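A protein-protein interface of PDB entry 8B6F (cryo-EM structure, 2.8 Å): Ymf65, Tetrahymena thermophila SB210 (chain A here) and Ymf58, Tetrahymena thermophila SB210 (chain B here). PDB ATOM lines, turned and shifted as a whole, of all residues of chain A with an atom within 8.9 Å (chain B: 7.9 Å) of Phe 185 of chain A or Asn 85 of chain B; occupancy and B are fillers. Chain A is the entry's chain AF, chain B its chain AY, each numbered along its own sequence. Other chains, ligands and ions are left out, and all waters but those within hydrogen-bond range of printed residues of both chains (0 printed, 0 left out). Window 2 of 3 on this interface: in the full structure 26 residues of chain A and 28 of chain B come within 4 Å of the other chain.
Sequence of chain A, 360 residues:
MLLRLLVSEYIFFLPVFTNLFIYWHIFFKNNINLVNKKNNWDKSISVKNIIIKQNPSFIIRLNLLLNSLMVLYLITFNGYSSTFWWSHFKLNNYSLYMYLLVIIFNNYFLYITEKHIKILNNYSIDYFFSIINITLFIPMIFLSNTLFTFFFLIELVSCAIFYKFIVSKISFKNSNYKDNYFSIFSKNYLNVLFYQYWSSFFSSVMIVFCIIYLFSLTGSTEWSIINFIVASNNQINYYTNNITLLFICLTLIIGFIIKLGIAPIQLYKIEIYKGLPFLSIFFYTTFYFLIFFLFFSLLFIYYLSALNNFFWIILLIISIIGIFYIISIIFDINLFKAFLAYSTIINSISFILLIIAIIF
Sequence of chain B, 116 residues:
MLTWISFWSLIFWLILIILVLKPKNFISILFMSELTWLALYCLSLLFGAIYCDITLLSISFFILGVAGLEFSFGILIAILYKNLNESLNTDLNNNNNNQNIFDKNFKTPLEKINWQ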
ATOM      1  N   ASP A 179      -9.976  32.429  42.158  1.00  0.00           N
ATOM      2  CA  ASP A 179      -9.146  31.526  41.369  1.00  0.00           C
ATOM      3  C   ASP A 179      -7.948  32.238  40.748  1.00  0.00           C
ATOM      4  O   ASP A 179      -7.437  31.810  39.711  1.00  0.00           O
ATOM      5  CB  ASP A 179      -9.983  30.861  40.280  1.00  0.00           C
ATOM      6  CG  ASP A 179     -11.167  30.103  40.840  1.00  0.00           C
ATOM      7  OD1 ASP A 179     -11.254  29.966  42.077  1.00  0.00           O
ATOM      8  OD2 ASP A 179     -12.015  29.649  40.044  1.00  0.00           O
ATOM      9  N   PHE A 182      -4.900  29.712  41.346  1.00  0.00           N
ATOM     10  CA  PHE A 182      -5.208  28.293  41.267  1.00  0.00           C
ATOM     11  C   PHE A 182      -5.614  27.958  39.840  1.00  0.00           C
ATOM     12  O   PHE A 182      -6.196  28.786  39.135  1.00  0.00           O
ATOM     13  CB  PHE A 182      -6.324  27.902  42.243  1.00  0.00           C
ATOM     14  CG  PHE A 182      -6.466  26.421  42.437  1.00  0.00           C
ATOM     15  CD1 PHE A 182      -5.674  25.752  43.356  1.00  0.00           C
ATOM     16  CD2 PHE A 182      -7.397  25.698  41.713  1.00  0.00           C
ATOM     17  CE1 PHE A 182      -5.802  24.391  43.541  1.00  0.00           C
ATOM     18  CE2 PHE A 182      -7.530  24.335  41.893  1.00  0.00           C
ATOM     19  CZ  PHE A 182      -6.731  23.682  42.809  1.00  0.00           C
ATOM     20  N   SER A 183      -5.297  26.738  39.420  1.00  0.00           N
ATOM     21  CA  SER A 183      -5.573  26.287  38.062  1.00  0.00           C
ATOM     22  C   SER A 183      -6.958  25.656  38.010  1.00  0.00           C
ATOM     23  O   SER A 183      -7.235  24.693  38.731  1.00  0.00           O
ATOM     24  CB  SER A 183      -4.518  25.286  37.600  1.00  0.00           C
ATOM     25  OG  SER A 183      -3.231  25.873  37.590  1.00  0.00           O
ATOM     26  N   ILE A 184      -7.822  26.201  37.158  1.00  0.00           N
ATOM     27  CA  ILE A 184      -9.158  25.668  36.925  1.00  0.00           C
ATOM     28  C   ILE A 184      -9.187  25.103  35.514  1.00  0.00           C
ATOM     29  O   ILE A 184      -8.803  25.785  34.556  1.00  0.00           O
ATOM     30  CB  ILE A 184     -10.239  26.747  37.107  1.00  0.00           C
ATOM     31  CG1 ILE A 184     -10.076  27.455  38.453  1.00  0.00           C
ATOM     32  CG2 ILE A 184     -11.626  26.133  36.990  1.00  0.00           C
ATOM     33  CD1 ILE A 184     -10.144  26.539  39.654  1.00  0.00           C
ATOM     34  N   PHE A 185      -9.643  23.863  35.385  1.00  0.00           N
ATOM     35  CA  PHE A 185      -9.626  23.149  34.118  1.00  0.00           C
ATOM     36  C   PHE A 185     -11.034  23.113  33.539  1.00  0.00           C
ATOM     37  O   PHE A 185     -11.972  22.655  34.200  1.00  0.00           O
ATOM     38  CB  PHE A 185      -9.083  21.736  34.304  1.00  0.00           C
ATOM     39  CG  PHE A 185      -7.783  21.684  35.044  1.00  0.00           C
ATOM     40  CD1 PHE A 185      -6.608  22.088  34.435  1.00  0.00           C
ATOM     41  CD2 PHE A 185      -7.736  21.230  36.349  1.00  0.00           C
ATOM     42  CE1 PHE A 185      -5.410  22.042  35.117  1.00  0.00           C
ATOM     43  CE2 PHE A 185      -6.543  21.182  37.036  1.00  0.00           C
ATOM     44  CZ  PHE A 185      -5.379  21.587  36.419  1.00  0.00           C
ATOM     45  N   SER A 186     -11.176  23.595  32.307  1.00  0.00           N
ATOM     46  CA  SER A 186     -12.436  23.573  31.576  1.00  0.00           C
ATOM     47  C   SER A 186     -12.187  22.914  30.229  1.00  0.00           C
ATOM     48  O   SER A 186     -11.332  23.371  29.464  1.00  0.00           O
ATOM     49  CB  SER A 186     -12.991  24.988  31.394  1.00  0.00           C
ATOM     50  OG  SER A 186     -14.206  24.970  30.667  1.00  0.00           O
ATOM     51  N   LYS A 187     -12.930  21.847  29.939  1.00  0.00           N
ATOM     52  CA  LYS A 187     -12.722  21.051  28.738  1.00  0.00           C
ATOM     53  C   LYS A 187     -13.757  21.321  27.657  1.00  0.00           C
ATOM     54  O   LYS A 187     -13.780  20.611  26.648  1.00  0.00           O
ATOM     55  CB  LYS A 187     -12.730  19.560  29.077  1.00  0.00           C
ATOM     56  CG  LYS A 187     -11.455  19.046  29.711  1.00  0.00           C
ATOM     57  CD  LYS A 187     -11.329  19.453  31.163  1.00  0.00           C
ATOM     58  CE  LYS A 187     -10.096  18.822  31.786  1.00  0.00           C
ATOM     59  NZ  LYS A 187     -10.130  18.927  33.262  1.00  0.00           N
ATOM     60  N   ASN A 188     -14.613  22.325  27.840  1.00  0.00           N
ATOM     61  CA  ASN A 188     -15.701  22.542  26.892  1.00  0.00           C
ATOM     62  C   ASN A 188     -15.164  22.882  25.509  1.00  0.00           C
ATOM     63  O   ASN A 188     -15.658  22.370  24.500  1.00  0.00           O
ATOM     64  CB  ASN A 188     -16.625  23.645  27.399  1.00  0.00           C
ATOM     65  CG  ASN A 188     -17.329  23.262  28.677  1.00  0.00           C
ATOM     66  OD1 ASN A 188     -18.382  22.629  28.654  1.00  0.00           O
ATOM     67  ND2 ASN A 188     -16.748  23.641  29.808  1.00  0.00           N
ATOM     68  N   TYR A 189     -14.144  23.733  25.444  1.00  0.00           N
ATOM     69  CA  TYR A 189     -13.576  24.118  24.159  1.00  0.00           C
ATOM     70  C   TYR A 189     -13.063  22.898  23.401  1.00  0.00           C
ATOM     71  O   TYR A 189     -13.393  22.700  22.226  1.00  0.00           O
ATOM     72  CB  TYR A 189     -12.460  25.140  24.383  1.00  0.00           C
ATOM     73  CG  TYR A 189     -11.994  25.864  23.140  1.00  0.00           C
ATOM     74  CD1 TYR A 189     -12.838  26.728  22.457  1.00  0.00           C
ATOM     75  CD2 TYR A 189     -10.693  25.720  22.681  1.00  0.00           C
ATOM     76  CE1 TYR A 189     -12.409  27.403  21.332  1.00  0.00           C
ATOM     77  CE2 TYR A 189     -10.255  26.392  21.560  1.00  0.00           C
ATOM     78  CZ  TYR A 189     -11.116  27.234  20.892  1.00  0.00           C
ATOM     79  OH  TYR A 189     -10.684  27.905  19.774  1.00  0.00           O
ATOM     80  N   LEU A 190     -12.256  22.065  24.057  1.00  0.00           N
ATOM     81  CA  LEU A 190     -11.713  20.886  23.388  1.00  0.00           C
ATOM     82  C   LEU A 190     -12.812  19.906  23.008  1.00  0.00           C
ATOM     83  O   LEU A 190     -12.772  19.303  21.930  1.00  0.00           O
ATOM     84  CB  LEU A 190     -10.699  20.176  24.278  1.00  0.00           C
ATOM     85  CG  LEU A 190      -9.914  19.055  23.601  1.00  0.00           C
ATOM     86  CD1 LEU A 190      -9.103  19.583  22.430  1.00  0.00           C
ATOM     87  CD2 LEU A 190      -9.010  18.408  24.606  1.00  0.00           C
ATOM     88  N   ILE B  79      -2.121  19.804  19.646  1.00  0.00           N
ATOM     89  CA  ILE B  79      -1.284  20.755  20.371  1.00  0.00           C
ATOM     90  C   ILE B  79      -2.106  21.485  21.423  1.00  0.00           C
ATOM     91  O   ILE B  79      -1.634  21.742  22.535  1.00  0.00           O
ATOM     92  CB  ILE B  79      -0.603  21.725  19.390  1.00  0.00           C
ATOM     93  CG1 ILE B  79       0.451  20.967  18.581  1.00  0.00           C
ATOM     94  CG2 ILE B  79       0.021  22.905  20.137  1.00  0.00           C
ATOM     95  CD1 ILE B  79       1.083  21.771  17.481  1.00  0.00           C
ATOM     96  N   LEU B  80      -3.347  21.830  21.086  1.00  0.00           N
ATOM     97  CA  LEU B  80      -4.221  22.501  22.035  1.00  0.00           C
ATOM     98  C   LEU B  80      -4.522  21.636  23.253  1.00  0.00           C
ATOM     99  O   LEU B  80      -4.882  22.172  24.305  1.00  0.00           O
ATOM    100  CB  LEU B  80      -5.510  22.911  21.323  1.00  0.00           C
ATOM    101  CG  LEU B  80      -6.587  23.526  22.206  1.00  0.00           C
ATOM    102  CD1 LEU B  80      -6.154  24.876  22.770  1.00  0.00           C
ATOM    103  CD2 LEU B  80      -7.901  23.653  21.457  1.00  0.00           C
ATOM    104  N   TYR B  81      -4.395  20.314  23.131  1.00  0.00           N
ATOM    105  CA  TYR B  81      -4.577  19.432  24.280  1.00  0.00           C
ATOM    106  C   TYR B  81      -3.735  19.880  25.471  1.00  0.00           C
ATOM    107  O   TYR B  81      -4.194  19.838  26.618  1.00  0.00           O
ATOM    108  CB  TYR B  81      -4.223  17.993  23.897  1.00  0.00           C
ATOM    109  CG  TYR B  81      -5.412  17.121  23.565  1.00  0.00           C
ATOM    110  CD1 TYR B  81      -5.970  17.125  22.294  1.00  0.00           C
ATOM    111  CD2 TYR B  81      -5.961  16.277  24.518  1.00  0.00           C
ATOM    112  CE1 TYR B  81      -7.052  16.324  21.988  1.00  0.00           C
ATOM    113  CE2 TYR B  81      -7.039  15.470  24.223  1.00  0.00           C
ATOM    114  CZ  TYR B  81      -7.580  15.497  22.956  1.00  0.00           C
ATOM    115  OH  TYR B  81      -8.656  14.696  22.661  1.00  0.00           O
ATOM    116  N   LYS B  82      -2.497  20.309  25.218  1.00  0.00           N
ATOM    117  CA  LYS B  82      -1.610  20.718  26.304  1.00  0.00           C
ATOM    118  C   LYS B  82      -2.183  21.895  27.083  1.00  0.00           C
ATOM    119  O   LYS B  82      -2.288  21.845  28.313  1.00  0.00           O
ATOM    120  CB  LYS B  82      -0.228  21.071  25.749  1.00  0.00           C
ATOM    121  CG  LYS B  82       0.758  21.536  26.817  1.00  0.00           C
ATOM    122  CD  LYS B  82       2.115  21.890  26.229  1.00  0.00           C
ATOM    123  CE  LYS B  82       2.048  23.144  25.377  1.00  0.00           C
ATOM    124  NZ  LYS B  82       3.397  23.558  24.901  1.00  0.00           N
ATOM    125  N   ASN B  83      -2.557  22.971  26.389  1.00  0.00           N
ATOM    126  CA  ASN B  83      -3.073  24.141  27.091  1.00  0.00           C
ATOM    127  C   ASN B  83      -4.387  23.845  27.800  1.00  0.00           C
ATOM    128  O   ASN B  83      -4.705  24.491  28.803  1.00  0.00           O
ATOM    129  CB  ASN B  83      -3.251  25.299  26.110  1.00  0.00           C
ATOM    130  CG  ASN B  83      -2.022  26.177  26.018  1.00  0.00           C
ATOM    131  OD1 ASN B  83      -0.924  25.762  26.378  1.00  0.00           O
ATOM    132  ND2 ASN B  83      -2.203  27.398  25.534  1.00  0.00           N
ATOM    133  N   LEU B  84      -5.160  22.888  27.304  1.00  0.00           N
ATOM    134  CA  LEU B  84      -6.414  22.510  27.940  1.00  0.00           C
ATOM    135  C   LEU B  84      -6.242  21.433  29.004  1.00  0.00           C
ATOM    136  O   LEU B  84      -7.222  21.071  29.661  1.00  0.00           O
ATOM    137  CB  LEU B  84      -7.415  22.070  26.870  1.00  0.00           C
ATOM    138  CG  LEU B  84      -8.265  23.264  26.426  1.00  0.00           C
ATOM    139  CD1 LEU B  84      -8.635  23.195  24.987  1.00  0.00           C
ATOM    140  CD2 LEU B  84      -9.521  23.318  27.263  1.00  0.00           C
ATOM    141  N   ASN B  85      -5.025  20.927  29.199  1.00  0.00           N
ATOM    142  CA  ASN B  85      -4.737  19.961  30.259  1.00  0.00           C
ATOM    143  C   ASN B  85      -5.560  18.687  30.081  1.00  0.00           C
ATOM    144  O   ASN B  85      -6.271  18.245  30.985  1.00  0.00           O
ATOM    145  CB  ASN B  85      -4.971  20.580  31.636  1.00  0.00           C
ATOM    146  CG  ASN B  85      -4.548  19.661  32.763  1.00  0.00           C
ATOM    147  OD1 ASN B  85      -5.366  18.947  33.338  1.00  0.00           O
ATOM    148  ND2 ASN B  85      -3.260  19.671  33.080  1.00  0.00           N
ATOM    149  N   GLU B  86      -5.461  18.095  28.896  1.00  0.00           N
ATOM    150  CA  GLU B  86      -6.140  16.849  28.581  1.00  0.00           C
ATOM    151  C   GLU B  86      -5.119  15.839  28.091  1.00  0.00           C
ATOM    152  O   GLU B  86      -4.274  16.161  27.250  1.00  0.00           O
ATOM    153  CB  GLU B  86      -7.222  17.064  27.521  1.00  0.00           C
ATOM    154  CG  GLU B  86      -8.500  17.687  28.055  1.00  0.00           C
ATOM    155  CD  GLU B  86      -9.303  16.732  28.913  1.00  0.00           C
ATOM    156  OE1 GLU B  86      -8.853  16.401  30.029  1.00  0.00           O
ATOM    157  OE2 GLU B  86     -10.386  16.302  28.464  1.00  0.00           O
ATOM    158  N   SER B  87      -5.189  14.624  28.625  1.00  0.00           N
ATOM    159  CA  SER B  87      -4.329  13.555  28.148  1.00  0.00           C
ATOM    160  C   SER B  87      -4.727  13.163  26.733  1.00  0.00           C
ATOM    161  O   SER B  87      -5.912  13.095  26.401  1.00  0.00           O
ATOM    162  CB  SER B  87      -4.425  12.345  29.075  1.00  0.00           C
ATOM    163  OG  SER B  87      -3.531  11.321  28.679  1.00  0.00           O
ATOM    164  N   LEU B  88      -3.724  12.916  25.889  1.00  0.00           N
ATOM    165  CA  LEU B  88      -4.012  12.447  24.540  1.00  0.00           C
ATOM    166  C   LEU B  88      -4.792  11.143  24.569  1.00  0.00           C
ATOM    167  O   LEU B  88      -5.649  10.912  23.708  1.00  0.00           O
ATOM    168  CB  LEU B  88      -2.713  12.280  23.752  1.00  0.00           C
ATOM    169  CG  LEU B  88      -1.977  13.577  23.405  1.00  0.00           C
ATOM    170  CD1 LEU B  88      -0.623  13.272  22.794  1.00  0.00           C
ATOM    171  CD2 LEU B  88      -2.798  14.441  22.462  1.00  0.00           C
ATOM    172  N   ASN B  93      -9.208  10.747  30.694  1.00  0.00           N
ATOM    173  CA  ASN B  93      -9.829  12.023  31.018  1.00  0.00           C
ATOM    174  C   ASN B  93     -11.116  11.867  31.814  1.00  0.00           C
ATOM    175  O   ASN B  93     -11.777  12.870  32.097  1.00  0.00           O
ATOM    176  CB  ASN B  93     -10.118  12.809  29.734  1.00  0.00           C
ATOM    177  CG  ASN B  93      -8.857  13.179  28.983  1.00  0.00           C
ATOM    178  OD1 ASN B  93      -7.789  13.325  29.575  1.00  0.00           O
ATOM    179  ND2 ASN B  93      -8.974  13.336  27.670  1.00  0.00           N
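Of chain B, only Asn 85 comes within 4 Å of Phe 185 of chain A.
Of the printed residues of chain B, Lys 187 of chain A touches Asn 85 (3.95 Å) and Glu 86 (3.2 Å).
Of the printed residues of chain A, Tyr 81 of chain B touches Leu 190.
Printed residues of chain B within 4 Å of Leu 190 of chain A: Tyr 81 (3.6 Å), Leu 84 (3.7 Å) and Glu 86 (3.6 Å).
Of the printed residues of chain B, Ser 186 of chain A touches Leu 84 (2.9 Å).
Printed residues of chain A within 4 Å of Leu 80 of chain B: Tyr 189.
Asn 83 of chain B touches none of the printed residues of chain A.
The nearest residue of chain B that does not touch Phe 185 of chain A is Leu 84 of chain B (4.9 Å).
The nearest residue of chain A that does not touch Asn 85 of chain B is Leu 190 of chain A (6.5 Å).
The nearest printed residue of chain B that does not touch Tyr 189 of chain A is Asn 83 of chain B (8.2 Å).
The side-chain hydroxyl (OG) of Ser 186 of chain A sits at hydrogen-bond distance from the side-chain amide nitrogen (ND2) of Asn 188 of chain A (3.0 Å).
N of Glu 86 of chain B sits at hydrogen-bond distance from O of Tyr 81 of chain B (3.1 Å).
The side-chain carboxylate (OE1) of Glu 86 of chain B sits close to the side-chain amide oxygen (OD1) of Asn 93 of chain B, 3.3 Å away.
Of the 11 printed residues of chain B, 5 touch a printed residue of chain A.
Printed residues of chain B that touch a printed residue of chain A: Leu 80, Tyr 81, Leu 84, Asn 85 and Glu 86.
Hydrophobic or aromatic side chains of chain B within 4 Å of the printed part of chain A: Leu 80, Tyr 81 and Leu 84.
Hydrophobic or aromatic side chains of chain A that line the printed part of chain B: Phe 185, Tyr 189 and Leu 190.
Along chain A the printed residues that touch a printed residue of chain B span positions 185 to 190.
Among the printed residues, pairs that only touch across the chains: Ser 186 of chain A with Leu 84 of chain B (2.9 Å), Lys 187 of chain A with Glu 86 of chain B (3.2 Å), Phe 185 of chain A with Asn 85 of chain B (3.5 Å), Leu 190 of chain A with Tyr 81 of chain B (3.6 Å), Leu 190 of chain A with Glu 86 of chain B (3.6 Å), Tyr 189 of chain A with Leu 80 of chain B (3.6 Å), Leu 190 of chain A with Leu 84 of chain B (3.7 Å), Lys 187 of chain A with Asn 85 of chain B (3.95 Å) and Tyr 189 of chain A with Leu 84 of chain B (3.99 Å).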
